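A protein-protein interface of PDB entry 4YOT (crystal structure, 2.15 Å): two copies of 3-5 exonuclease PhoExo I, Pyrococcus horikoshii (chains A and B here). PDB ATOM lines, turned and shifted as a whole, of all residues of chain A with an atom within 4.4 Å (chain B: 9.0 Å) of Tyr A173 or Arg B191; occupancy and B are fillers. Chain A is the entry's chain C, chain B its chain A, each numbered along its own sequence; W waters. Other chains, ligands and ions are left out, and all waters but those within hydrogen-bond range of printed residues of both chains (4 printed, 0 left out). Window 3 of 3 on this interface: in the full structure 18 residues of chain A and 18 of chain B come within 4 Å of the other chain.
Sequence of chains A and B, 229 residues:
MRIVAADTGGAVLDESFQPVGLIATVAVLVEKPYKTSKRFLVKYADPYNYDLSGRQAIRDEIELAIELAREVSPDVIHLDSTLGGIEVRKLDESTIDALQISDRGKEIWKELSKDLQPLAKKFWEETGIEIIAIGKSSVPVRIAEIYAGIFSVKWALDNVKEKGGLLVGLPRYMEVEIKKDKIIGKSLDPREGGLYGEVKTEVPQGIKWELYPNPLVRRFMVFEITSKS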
ATOM      1  N   ARG A 142      -7.952  10.363   7.958  1.00  0.00           N
ATOM      2  CA  ARG A 142      -8.907  11.406   8.326  1.00  0.00           C
ATOM      3  C   ARG A 142      -8.199  12.708   8.717  1.00  0.00           C
ATOM      4  O   ARG A 142      -8.670  13.802   8.401  1.00  0.00           O
ATOM      5  CB  ARG A 142      -9.802  10.925   9.467  1.00  0.00           C
ATOM      6  CG  ARG A 142     -10.727  11.992  10.060  1.00  0.00           C
ATOM      7  CD  ARG A 142     -11.767  12.508   9.067  1.00  0.00           C
ATOM      8  NE  ARG A 142     -12.749  13.373   9.725  1.00  0.00           N
ATOM      9  CZ  ARG A 142     -13.525  14.243   9.085  1.00  0.00           C
ATOM     10  NH1 ARG A 142     -13.437  14.375   7.766  1.00  0.00           N
ATOM     11  NH2 ARG A 142     -14.384  14.990   9.762  1.00  0.00           N
ATOM     12  N   PRO A 171     -14.239  19.130   3.301  1.00  0.00           N
ATOM     13  CA  PRO A 171     -14.432  17.695   3.545  1.00  0.00           C
ATOM     14  C   PRO A 171     -15.515  17.459   4.597  1.00  0.00           C
ATOM     15  O   PRO A 171     -15.800  18.373   5.381  1.00  0.00           O
ATOM     16  CB  PRO A 171     -13.076  17.254   4.098  1.00  0.00           C
ATOM     17  CG  PRO A 171     -12.089  18.207   3.466  1.00  0.00           C
ATOM     18  CD  PRO A 171     -12.815  19.524   3.373  1.00  0.00           C
ATOM     19  N   ARG A 172     -16.081  16.253   4.629  1.00  0.00           N
ATOM     20  CA  ARG A 172     -17.268  15.973   5.441  1.00  0.00           C
ATOM     21  C   ARG A 172     -17.098  16.358   6.904  1.00  0.00           C
ATOM     22  O   ARG A 172     -16.023  16.196   7.481  1.00  0.00           O
ATOM     23  CB  ARG A 172     -17.717  14.506   5.300  1.00  0.00           C
ATOM     24  CG  ARG A 172     -16.840  13.483   6.013  1.00  0.00           C
ATOM     25  CD  ARG A 172     -17.233  12.048   5.657  1.00  0.00           C
ATOM     26  NE  ARG A 172     -16.779  11.680   4.319  1.00  0.00           N
ATOM     27  CZ  ARG A 172     -17.586  11.338   3.322  1.00  0.00           C
ATOM     28  NH1 ARG A 172     -18.899  11.301   3.510  1.00  0.00           N
ATOM     29  NH2 ARG A 172     -17.085  11.026   2.135  1.00  0.00           N
ATOM     30  N   TYR A 173     -18.177  16.888   7.469  1.00  0.00           N
ATOM     31  CA  TYR A 173     -18.249  17.351   8.856  1.00  0.00           C
ATOM     32  C   TYR A 173     -16.966  17.835   9.524  1.00  0.00           C
ATOM     33  O   TYR A 173     -16.495  17.255  10.513  1.00  0.00           O
ATOM     34  CB  TYR A 173     -18.982  16.348   9.752  1.00  0.00           C
ATOM     35  CG  TYR A 173     -18.608  14.895   9.593  1.00  0.00           C
ATOM     36  CD1 TYR A 173     -17.532  14.347  10.284  1.00  0.00           C
ATOM     37  CD2 TYR A 173     -19.369  14.057   8.791  1.00  0.00           C
ATOM     38  CE1 TYR A 173     -17.213  13.006  10.152  1.00  0.00           C
ATOM     39  CE2 TYR A 173     -19.066  12.727   8.659  1.00  0.00           C
ATOM     40  CZ  TYR A 173     -17.992  12.205   9.338  1.00  0.00           C
ATOM     41  OH  TYR A 173     -17.700  10.872   9.187  1.00  0.00           O
ATOM     42  N   MET A 174     -16.409  18.910   8.991  1.00  0.00           N
ATOM     43  CA  MET A 174     -15.327  19.583   9.690  1.00  0.00           C
ATOM     44  C   MET A 174     -15.580  21.073   9.638  1.00  0.00           C
ATOM     45  O   MET A 174     -16.277  21.561   8.742  1.00  0.00           O
ATOM     46  CB  MET A 174     -13.972  19.241   9.080  1.00  0.00           C
ATOM     47  CG  MET A 174     -13.766  19.803   7.685  1.00  0.00           C
ATOM     48  SD  MET A 174     -12.050  19.646   7.170  1.00  0.00           S
ATOM     49  CE  MET A 174     -11.288  20.896   8.204  1.00  0.00           C
ATOM     50  N   SER A 187     -12.645  18.231  13.434  1.00  0.00           N
ATOM     51  CA  SER A 187     -13.759  17.365  13.058  1.00  0.00           C
ATOM     52  C   SER A 187     -14.972  17.761  13.879  1.00  0.00           C
ATOM     53  O   SER A 187     -14.847  18.077  15.064  1.00  0.00           O
ATOM     54  CB  SER A 187     -13.417  15.899  13.318  1.00  0.00           C
ATOM     55  OG  SER A 187     -14.483  15.046  12.925  1.00  0.00           O
ATOM     56  N   LEU A 188     -16.140  17.758  13.250  1.00  0.00           N
ATOM     57  CA  LEU A 188     -17.378  18.041  13.960  1.00  0.00           C
ATOM     58  C   LEU A 188     -17.946  16.770  14.584  1.00  0.00           C
ATOM     59  O   LEU A 188     -18.951  16.822  15.295  1.00  0.00           O
ATOM     60  CB  LEU A 188     -18.406  18.676  13.023  1.00  0.00           C
ATOM     61  CG  LEU A 188     -18.168  20.126  12.605  1.00  0.00           C
ATOM     62  CD1 LEU A 188     -19.226  20.560  11.612  1.00  0.00           C
ATOM     63  CD2 LEU A 188     -18.169  21.037  13.828  1.00  0.00           C
ATOM     64  N   ASP A 189     -17.305  15.633  14.316  1.00  0.00           N
ATOM     65  CA  ASP A 189     -17.761  14.359  14.869  1.00  0.00           C
ATOM     66  C   ASP A 189     -16.986  13.983  16.126  1.00  0.00           C
ATOM     67  O   ASP A 189     -15.842  13.537  16.040  1.00  0.00           O
ATOM     68  CB  ASP A 189     -17.641  13.239  13.836  1.00  0.00           C
ATOM     69  CG  ASP A 189     -18.353  11.961  14.273  1.00  0.00           C
ATOM     70  OD1 ASP A 189     -19.068  11.981  15.299  1.00  0.00           O
ATOM     71  OD2 ASP A 189     -18.209  10.935  13.580  1.00  0.00           O
ATOM     72  N   ARG A 191     -17.335  11.487  17.873  1.00  0.00           N
ATOM     73  CA  ARG A 191     -17.051  10.053  17.849  1.00  0.00           C
ATOM     74  C   ARG A 191     -15.620   9.760  17.379  1.00  0.00           C
ATOM     75  O   ARG A 191     -15.054   8.716  17.709  1.00  0.00           O
ATOM     76  CB  ARG A 191     -18.052   9.319  16.953  1.00  0.00           C
ATOM     77  CG  ARG A 191     -19.501   9.464  17.374  1.00  0.00           C
ATOM     78  CD  ARG A 191     -20.425   8.763  16.376  1.00  0.00           C
ATOM     79  NE  ARG A 191     -20.186   9.222  15.009  1.00  0.00           N
ATOM     80  CZ  ARG A 191     -20.562   8.559  13.917  1.00  0.00           C
ATOM     81  NH1 ARG A 191     -21.201   7.400  14.019  1.00  0.00           N
ATOM     82  NH2 ARG A 191     -20.295   9.055  12.715  1.00  0.00           N
ATOM     83  N   GLU A 192     -15.035  10.684  16.618  1.00  0.00           N
ATOM     84  CA  GLU A 192     -13.670  10.501  16.117  1.00  0.00           C
ATOM     85  C   GLU A 192     -12.612  10.793  17.188  1.00  0.00           C
ATOM     86  O   GLU A 192     -11.432  10.474  17.009  1.00  0.00           O
ATOM     87  CB  GLU A 192     -13.441  11.305  14.822  1.00  0.00           C
ATOM     88  CG  GLU A 192     -14.323  10.822  13.649  1.00  0.00           C
ATOM     89  CD  GLU A 192     -13.960  11.434  12.289  1.00  0.00           C
ATOM     90  OE1 GLU A 192     -14.140  10.738  11.267  1.00  0.00           O
ATOM     91  OE2 GLU A 192     -13.521  12.606  12.230  1.00  0.00           O
ATOM     92  N   ARG A 219     -24.298  17.515   6.367  1.00  0.00           N
ATOM     93  CA  ARG A 219     -23.038  17.200   7.069  1.00  0.00           C
ATOM     94  C   ARG A 219     -21.760  17.706   6.370  1.00  0.00           C
ATOM     95  O   ARG A 219     -20.648  17.355   6.768  1.00  0.00           O
ATOM     96  CB  ARG A 219     -22.923  15.702   7.398  1.00  0.00           C
ATOM     97  CG  ARG A 219     -23.995  15.188   8.346  1.00  0.00           C
ATOM     98  CD  ARG A 219     -23.771  13.720   8.688  1.00  0.00           C
ATOM     99  NE  ARG A 219     -23.836  12.874   7.503  1.00  0.00           N
ATOM    100  CZ  ARG A 219     -24.957  12.317   7.054  1.00  0.00           C
ATOM    101  NH1 ARG A 219     -26.100  12.511   7.699  1.00  0.00           N
ATOM    102  NH2 ARG A 219     -24.938  11.569   5.961  1.00  0.00           N
ATOM    103  N   MET A 221     -19.781  21.321   5.256  1.00  0.00           N
ATOM    104  CA  MET A 221     -19.781  22.760   5.491  1.00  0.00           C
ATOM    105  C   MET A 221     -19.173  23.513   4.309  1.00  0.00           C
ATOM    106  O   MET A 221     -18.437  22.943   3.500  1.00  0.00           O
ATOM    107  CB  MET A 221     -19.036  23.100   6.790  1.00  0.00           C
ATOM    108  CG  MET A 221     -19.553  22.356   8.020  1.00  0.00           C
ATOM    109  SD  MET A 221     -21.296  22.681   8.390  1.00  0.00           S
ATOM    110  CE  MET A 221     -21.976  21.021   8.305  1.00  0.00           C
ATOM    111  N   VAL B 139     -30.390  19.982   3.619  1.00  0.00           N
ATOM    112  CA  VAL B 139     -30.459  20.643   4.923  1.00  0.00           C
ATOM    113  C   VAL B 139     -31.852  21.254   5.176  1.00  0.00           C
ATOM    114  O   VAL B 139     -32.408  21.082   6.256  1.00  0.00           O
ATOM    115  CB  VAL B 139     -29.310  21.682   5.122  1.00  0.00           C
ATOM    116  CG1 VAL B 139     -29.500  22.482   6.401  1.00  0.00           C
ATOM    117  CG2 VAL B 139     -27.954  20.978   5.134  1.00  0.00           C
ATOM    118  N   ARG B 172     -35.445  11.701  14.142  1.00  0.00           N
ATOM    119  CA  ARG B 172     -34.152  11.161  14.543  1.00  0.00           C
ATOM    120  C   ARG B 172     -33.209  12.199  15.155  1.00  0.00           C
ATOM    121  O   ARG B 172     -33.170  13.350  14.724  1.00  0.00           O
ATOM    122  CB  ARG B 172     -33.479  10.438  13.369  1.00  0.00           C
ATOM    123  CG  ARG B 172     -32.860  11.339  12.323  1.00  0.00           C
ATOM    124  CD  ARG B 172     -32.417  10.538  11.112  1.00  0.00           C
ATOM    125  NE  ARG B 172     -33.559   9.934  10.427  1.00  0.00           N
ATOM    126  CZ  ARG B 172     -33.728   8.625  10.273  1.00  0.00           C
ATOM    127  NH1 ARG B 172     -32.816   7.782  10.736  1.00  0.00           N
ATOM    128  NH2 ARG B 172     -34.800   8.158   9.648  1.00  0.00           N
ATOM    129  N   TYR B 173     -32.478  11.759  16.175  1.00  0.00           N
ATOM    130  CA  TYR B 173     -31.505  12.567  16.921  1.00  0.00           C
ATOM    131  C   TYR B 173     -31.726  14.072  16.968  1.00  0.00           C
ATOM    132  O   TYR B 173     -30.915  14.860  16.460  1.00  0.00           O
ATOM    133  CB  TYR B 173     -30.067  12.217  16.538  1.00  0.00           C
ATOM    134  CG  TYR B 173     -29.761  12.095  15.060  1.00  0.00           C
ATOM    135  CD1 TYR B 173     -29.425  13.211  14.302  1.00  0.00           C
ATOM    136  CD2 TYR B 173     -29.746  10.853  14.440  1.00  0.00           C
ATOM    137  CE1 TYR B 173     -29.115  13.096  12.957  1.00  0.00           C
ATOM    138  CE2 TYR B 173     -29.430  10.727  13.104  1.00  0.00           C
ATOM    139  CZ  TYR B 173     -29.117  11.852  12.368  1.00  0.00           C
ATOM    140  OH  TYR B 173     -28.806  11.731  11.037  1.00  0.00           O
ATOM    141  N   SER B 187     -30.941  19.783  16.370  1.00  0.00           N
ATOM    142  CA  SER B 187     -30.345  18.500  16.026  1.00  0.00           C
ATOM    143  C   SER B 187     -29.362  18.119  17.121  1.00  0.00           C
ATOM    144  O   SER B 187     -28.706  18.981  17.702  1.00  0.00           O
ATOM    145  CB  SER B 187     -29.600  18.585  14.699  1.00  0.00           C
ATOM    146  OG  SER B 187     -29.061  17.320  14.358  1.00  0.00           O
ATOM    147  N   LEU B 188     -29.259  16.828  17.403  1.00  0.00           N
ATOM    148  CA  LEU B 188     -28.285  16.351  18.379  1.00  0.00           C
ATOM    149  C   LEU B 188     -26.985  15.954  17.675  1.00  0.00           C
ATOM    150  O   LEU B 188     -26.019  15.553  18.322  1.00  0.00           O
ATOM    151  CB  LEU B 188     -28.857  15.169  19.177  1.00  0.00           C
ATOM    152  CG  LEU B 188     -29.830  15.488  20.313  1.00  0.00           C
ATOM    153  CD1 LEU B 188     -30.406  14.211  20.869  1.00  0.00           C
ATOM    154  CD2 LEU B 188     -29.122  16.273  21.425  1.00  0.00           C
ATOM    155  N   ASP B 189     -26.966  16.065  16.346  1.00  0.00           N
ATOM    156  CA  ASP B 189     -25.783  15.703  15.574  1.00  0.00           C
ATOM    157  C   ASP B 189     -24.978  16.943  15.252  1.00  0.00           C
ATOM    158  O   ASP B 189     -25.373  17.722  14.383  1.00  0.00           O
ATOM    159  CB  ASP B 189     -26.185  15.032  14.262  1.00  0.00           C
ATOM    160  CG  ASP B 189     -25.017  14.344  13.578  1.00  0.00           C
ATOM    161  OD1 ASP B 189     -23.862  14.504  14.046  1.00  0.00           O
ATOM    162  OD2 ASP B 189     -25.256  13.638  12.574  1.00  0.00           O
ATOM    163  N   PRO B 190     -23.833  17.131  15.934  1.00  0.00           N
ATOM    164  CA  PRO B 190     -23.004  18.307  15.644  1.00  0.00           C
ATOM    165  C   PRO B 190     -22.456  18.292  14.220  1.00  0.00           C
ATOM    166  O   PRO B 190     -22.055  19.346  13.725  1.00  0.00           O
ATOM    167  CB  PRO B 190     -21.851  18.195  16.658  1.00  0.00           C
ATOM    168  CG  PRO B 190     -21.847  16.771  17.101  1.00  0.00           C
ATOM    169  CD  PRO B 190     -23.271  16.305  17.017  1.00  0.00           C
ATOM    170  N   ARG B 191     -22.447  17.129  13.572  1.00  0.00           N
ATOM    171  CA  ARG B 191     -21.961  17.033  12.198  1.00  0.00           C
ATOM    172  C   ARG B 191     -22.841  17.829  11.234  1.00  0.00           C
ATOM    173  O   ARG B 191     -22.398  18.214  10.152  1.00  0.00           O
ATOM    174  CB  ARG B 191     -21.879  15.574  11.749  1.00  0.00           C
ATOM    175  CG  ARG B 191     -20.981  14.703  12.615  1.00  0.00           C
ATOM    176  CD  ARG B 191     -20.978  13.259  12.130  1.00  0.00           C
ATOM    177  NE  ARG B 191     -22.336  12.743  12.008  1.00  0.00           N
ATOM    178  CZ  ARG B 191     -22.674  11.668  11.300  1.00  0.00           C
ATOM    179  NH1 ARG B 191     -21.753  10.976  10.644  1.00  0.00           N
ATOM    180  NH2 ARG B 191     -23.939  11.288  11.246  1.00  0.00           N
ATOM    181  N   GLU B 192     -24.083  18.089  11.634  1.00  0.00           N
ATOM    182  CA  GLU B 192     -25.006  18.834  10.784  1.00  0.00           C
ATOM    183  C   GLU B 192     -24.759  20.338  10.838  1.00  0.00           C
ATOM    184  O   GLU B 192     -25.354  21.099  10.069  1.00  0.00           O
ATOM    185  CB  GLU B 192     -26.463  18.485  11.122  1.00  0.00           C
ATOM    186  CG  GLU B 192     -26.806  17.049  10.764  1.00  0.00           C
ATOM    187  CD  GLU B 192     -28.285  16.704  10.924  1.00  0.00           C
ATOM    188  OE1 GLU B 192     -28.755  15.835  10.166  1.00  0.00           O
ATOM    189  OE2 GLU B 192     -28.968  17.271  11.808  1.00  0.00           O
ATOM    190  N   GLY B 193     -23.874  20.765  11.734  1.00  0.00           N
ATOM    191  CA  GLY B 193     -23.428  22.146  11.743  1.00  0.00           C
ATOM    192  C   GLY B 193     -24.313  23.093  12.528  1.00  0.00           C
ATOM    193  O   GLY B 193     -24.229  24.303  12.331  1.00  0.00           O
ATOM    194  N   GLY B 194     -25.159  22.554  13.409  1.00  0.00           N
ATOM    195  CA  GLY B 194     -25.922  23.388  14.326  1.00  0.00           C
ATOM    196  C   GLY B 194     -27.319  23.757  13.854  1.00  0.00           C
ATOM    197  O   GLY B 194     -27.745  24.906  13.976  1.00  0.00           O
ATOM    198  N   LEU B 195     -28.047  22.782  13.324  1.00  0.00           N
ATOM    199  CA  LEU B 195     -29.399  23.043  12.841  1.00  0.00           C
ATOM    200  C   LEU B 195     -30.391  23.151  14.009  1.00  0.00           C
ATOM    201  O   LEU B 195     -30.344  22.359  14.959  1.00  0.00           O
ATOM    202  CB  LEU B 195     -29.835  21.955  11.858  1.00  0.00           C
ATOM    203  CG  LEU B 195     -28.834  21.646  10.742  1.00  0.00           C
ATOM    204  CD1 LEU B 195     -29.391  20.593   9.821  1.00  0.00           C
ATOM    205  CD2 LEU B 195     -28.452  22.900   9.955  1.00  0.00           C
ATOM    206  N   ARG B 219     -30.857   6.387  19.018  1.00  0.00           N
ATOM    207  CA  ARG B 219     -30.718   7.725  18.409  1.00  0.00           C
ATOM    208  C   ARG B 219     -32.041   8.461  18.192  1.00  0.00           C
ATOM    209  O   ARG B 219     -32.065   9.524  17.564  1.00  0.00           O
ATOM    210  CB  ARG B 219     -29.894   7.693  17.113  1.00  0.00           C
ATOM    211  CG  ARG B 219     -28.486   7.165  17.319  1.00  0.00           C
ATOM    212  CD  ARG B 219     -27.634   7.299  16.069  1.00  0.00           C
ATOM    213  NE  ARG B 219     -28.148   6.487  14.975  1.00  0.00           N
ATOM    214  CZ  ARG B 219     -27.854   5.204  14.797  1.00  0.00           C
ATOM    215  NH1 ARG B 219     -27.049   4.578  15.649  1.00  0.00           N
ATOM    216  NH2 ARG B 219     -28.372   4.542  13.772  1.00  0.00           N
HETATM  217  O   HOH W   1     -21.966  12.558  16.013  1.00  0.00           O
HETATM  218  O   HOH W   2     -27.133  13.724  10.030  1.00  0.00           O
HETATM  219  O   HOH W   3     -25.697  19.857   7.528  1.00  0.00           O
HETATM  220  O   HOH W   4     -21.886  25.400  10.851  1.00  0.00           O
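Printed residues of chain B that touch a printed residue of chain A: Pro B190, Arg B191, Glu B192 and Gly B193. Hydrophobic or aromatic side chains of chain B that line the printed part of chain A: Pro B190. Of the 12 printed residues of chain A, 6 touch a printed residue of chain B. Printed residues of chain A that touch a printed residue of chain B: Tyr A173, Leu A188, Asp A189, Arg A191, Arg A219 and Met A221. Among the printed residues, no Asp or Glu carboxylate lies within 4 Å of a Lys or Arg side-chain nitrogen of the other chain.
The side-chain carboxylate of Asp B189 is in salt-bridge range of the guanidinium group of Arg B191. The side-chain hydroxyl (OG) of Ser B187 sits at hydrogen-bond distance from the side-chain carboxylate (OE2) of Glu B192 (2.6 Å). The guanidinium group (NH2) of Arg A142 is in hydrogen-bond range of the backbone carbonyl oxygen (O) of Tyr A173 (3.2 Å). The guanidinium group of Arg A191 lies within salt-bridge range of the side-chain carboxylate of Asp A189, at 2.9 Å. The backbone carbonyl oxygen (O) of Tyr A173 lies within hydrogen-bond range of the backbone NH (N) of Leu A188 (2.8 Å). OG of Ser A187 sits close to N of Asp A189 (3.2 Å).
The guanidinium group of Arg A191 sits close to the guanidinium group of Arg B191 (3.2 Å).
Water W2 lies within hydrogen-bond range of OE1 of Glu B192 (2.7 Å), OH of Tyr B173 (2.8 Å), NH1 of Arg A219 (2.8 Å) and OD2 of Asp B189 (3.2 Å). Water W3 lies within hydrogen-bond range of O of Glu B192 (2.8 Å) and N of Arg A219 (3.0 Å). Water W4 lies within hydrogen-bond range of O of Gly B193 (3.0 Å) and SD of Met A221 (3.7 Å). Water W1 bridges OD1 of Asp A189 and OD1 of Asp B189.
Among the printed residues, pairs that only touch across the chains: Tyr A173 with Arg B191 (3.6 Å), Leu A188 with Pro B190 (3.4 Å), Leu A188 with Arg B191 (3.9 Å), Asp A189 with Arg B191 (3.6 Å), Arg A219 with Arg B191 (3.3 Å), Met A221 with Arg B191 (3.4 Å), Met A221 with Glu B192 (3.8 Å) and Met A221 with Gly B193 (3.9 Å).
Arg B191 touches just these residues of chain A: Tyr A173 (3.6 Å), Leu A188 (3.9 Å), Asp A189 (3.6 Å), Arg A191 (3.2 Å), Arg A219 (3.3 Å) and Met A221 (3.4 Å). No residue of chain B comes within 4 Å of Ser A187. Printed residues of chain A within 4 Å of Gly B193: Met A221 (3.9 Å). Of the printed residues of chain B, Asp A189 touches Arg B191 (3.6 Å). Leu B195 touches none of the printed residues of chain A. The nearest residue of chain B that does not touch Tyr A173 is Glu B192 (5.7 Å). The nearest printed residue of chain A that does not touch Arg B191 is Met A174 (6.1 Å).
Tyr A173 touches Arg B191, but with the chains exchanged Arg A191 does not touch Tyr B173 (8.9 Å). Leu A188 touches Arg B191, but with the chains exchanged Arg A191 does not touch Leu B188 (9.0 Å). Asp A189 touches Arg B191, but with the chains exchanged Arg A191 does not touch Asp B189 (6.5 Å). Arg A191 touches its own counterpart, Arg B191. Positions printed for both chains: 172, 173, 187, 188, 189, 191, 192 and 219.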
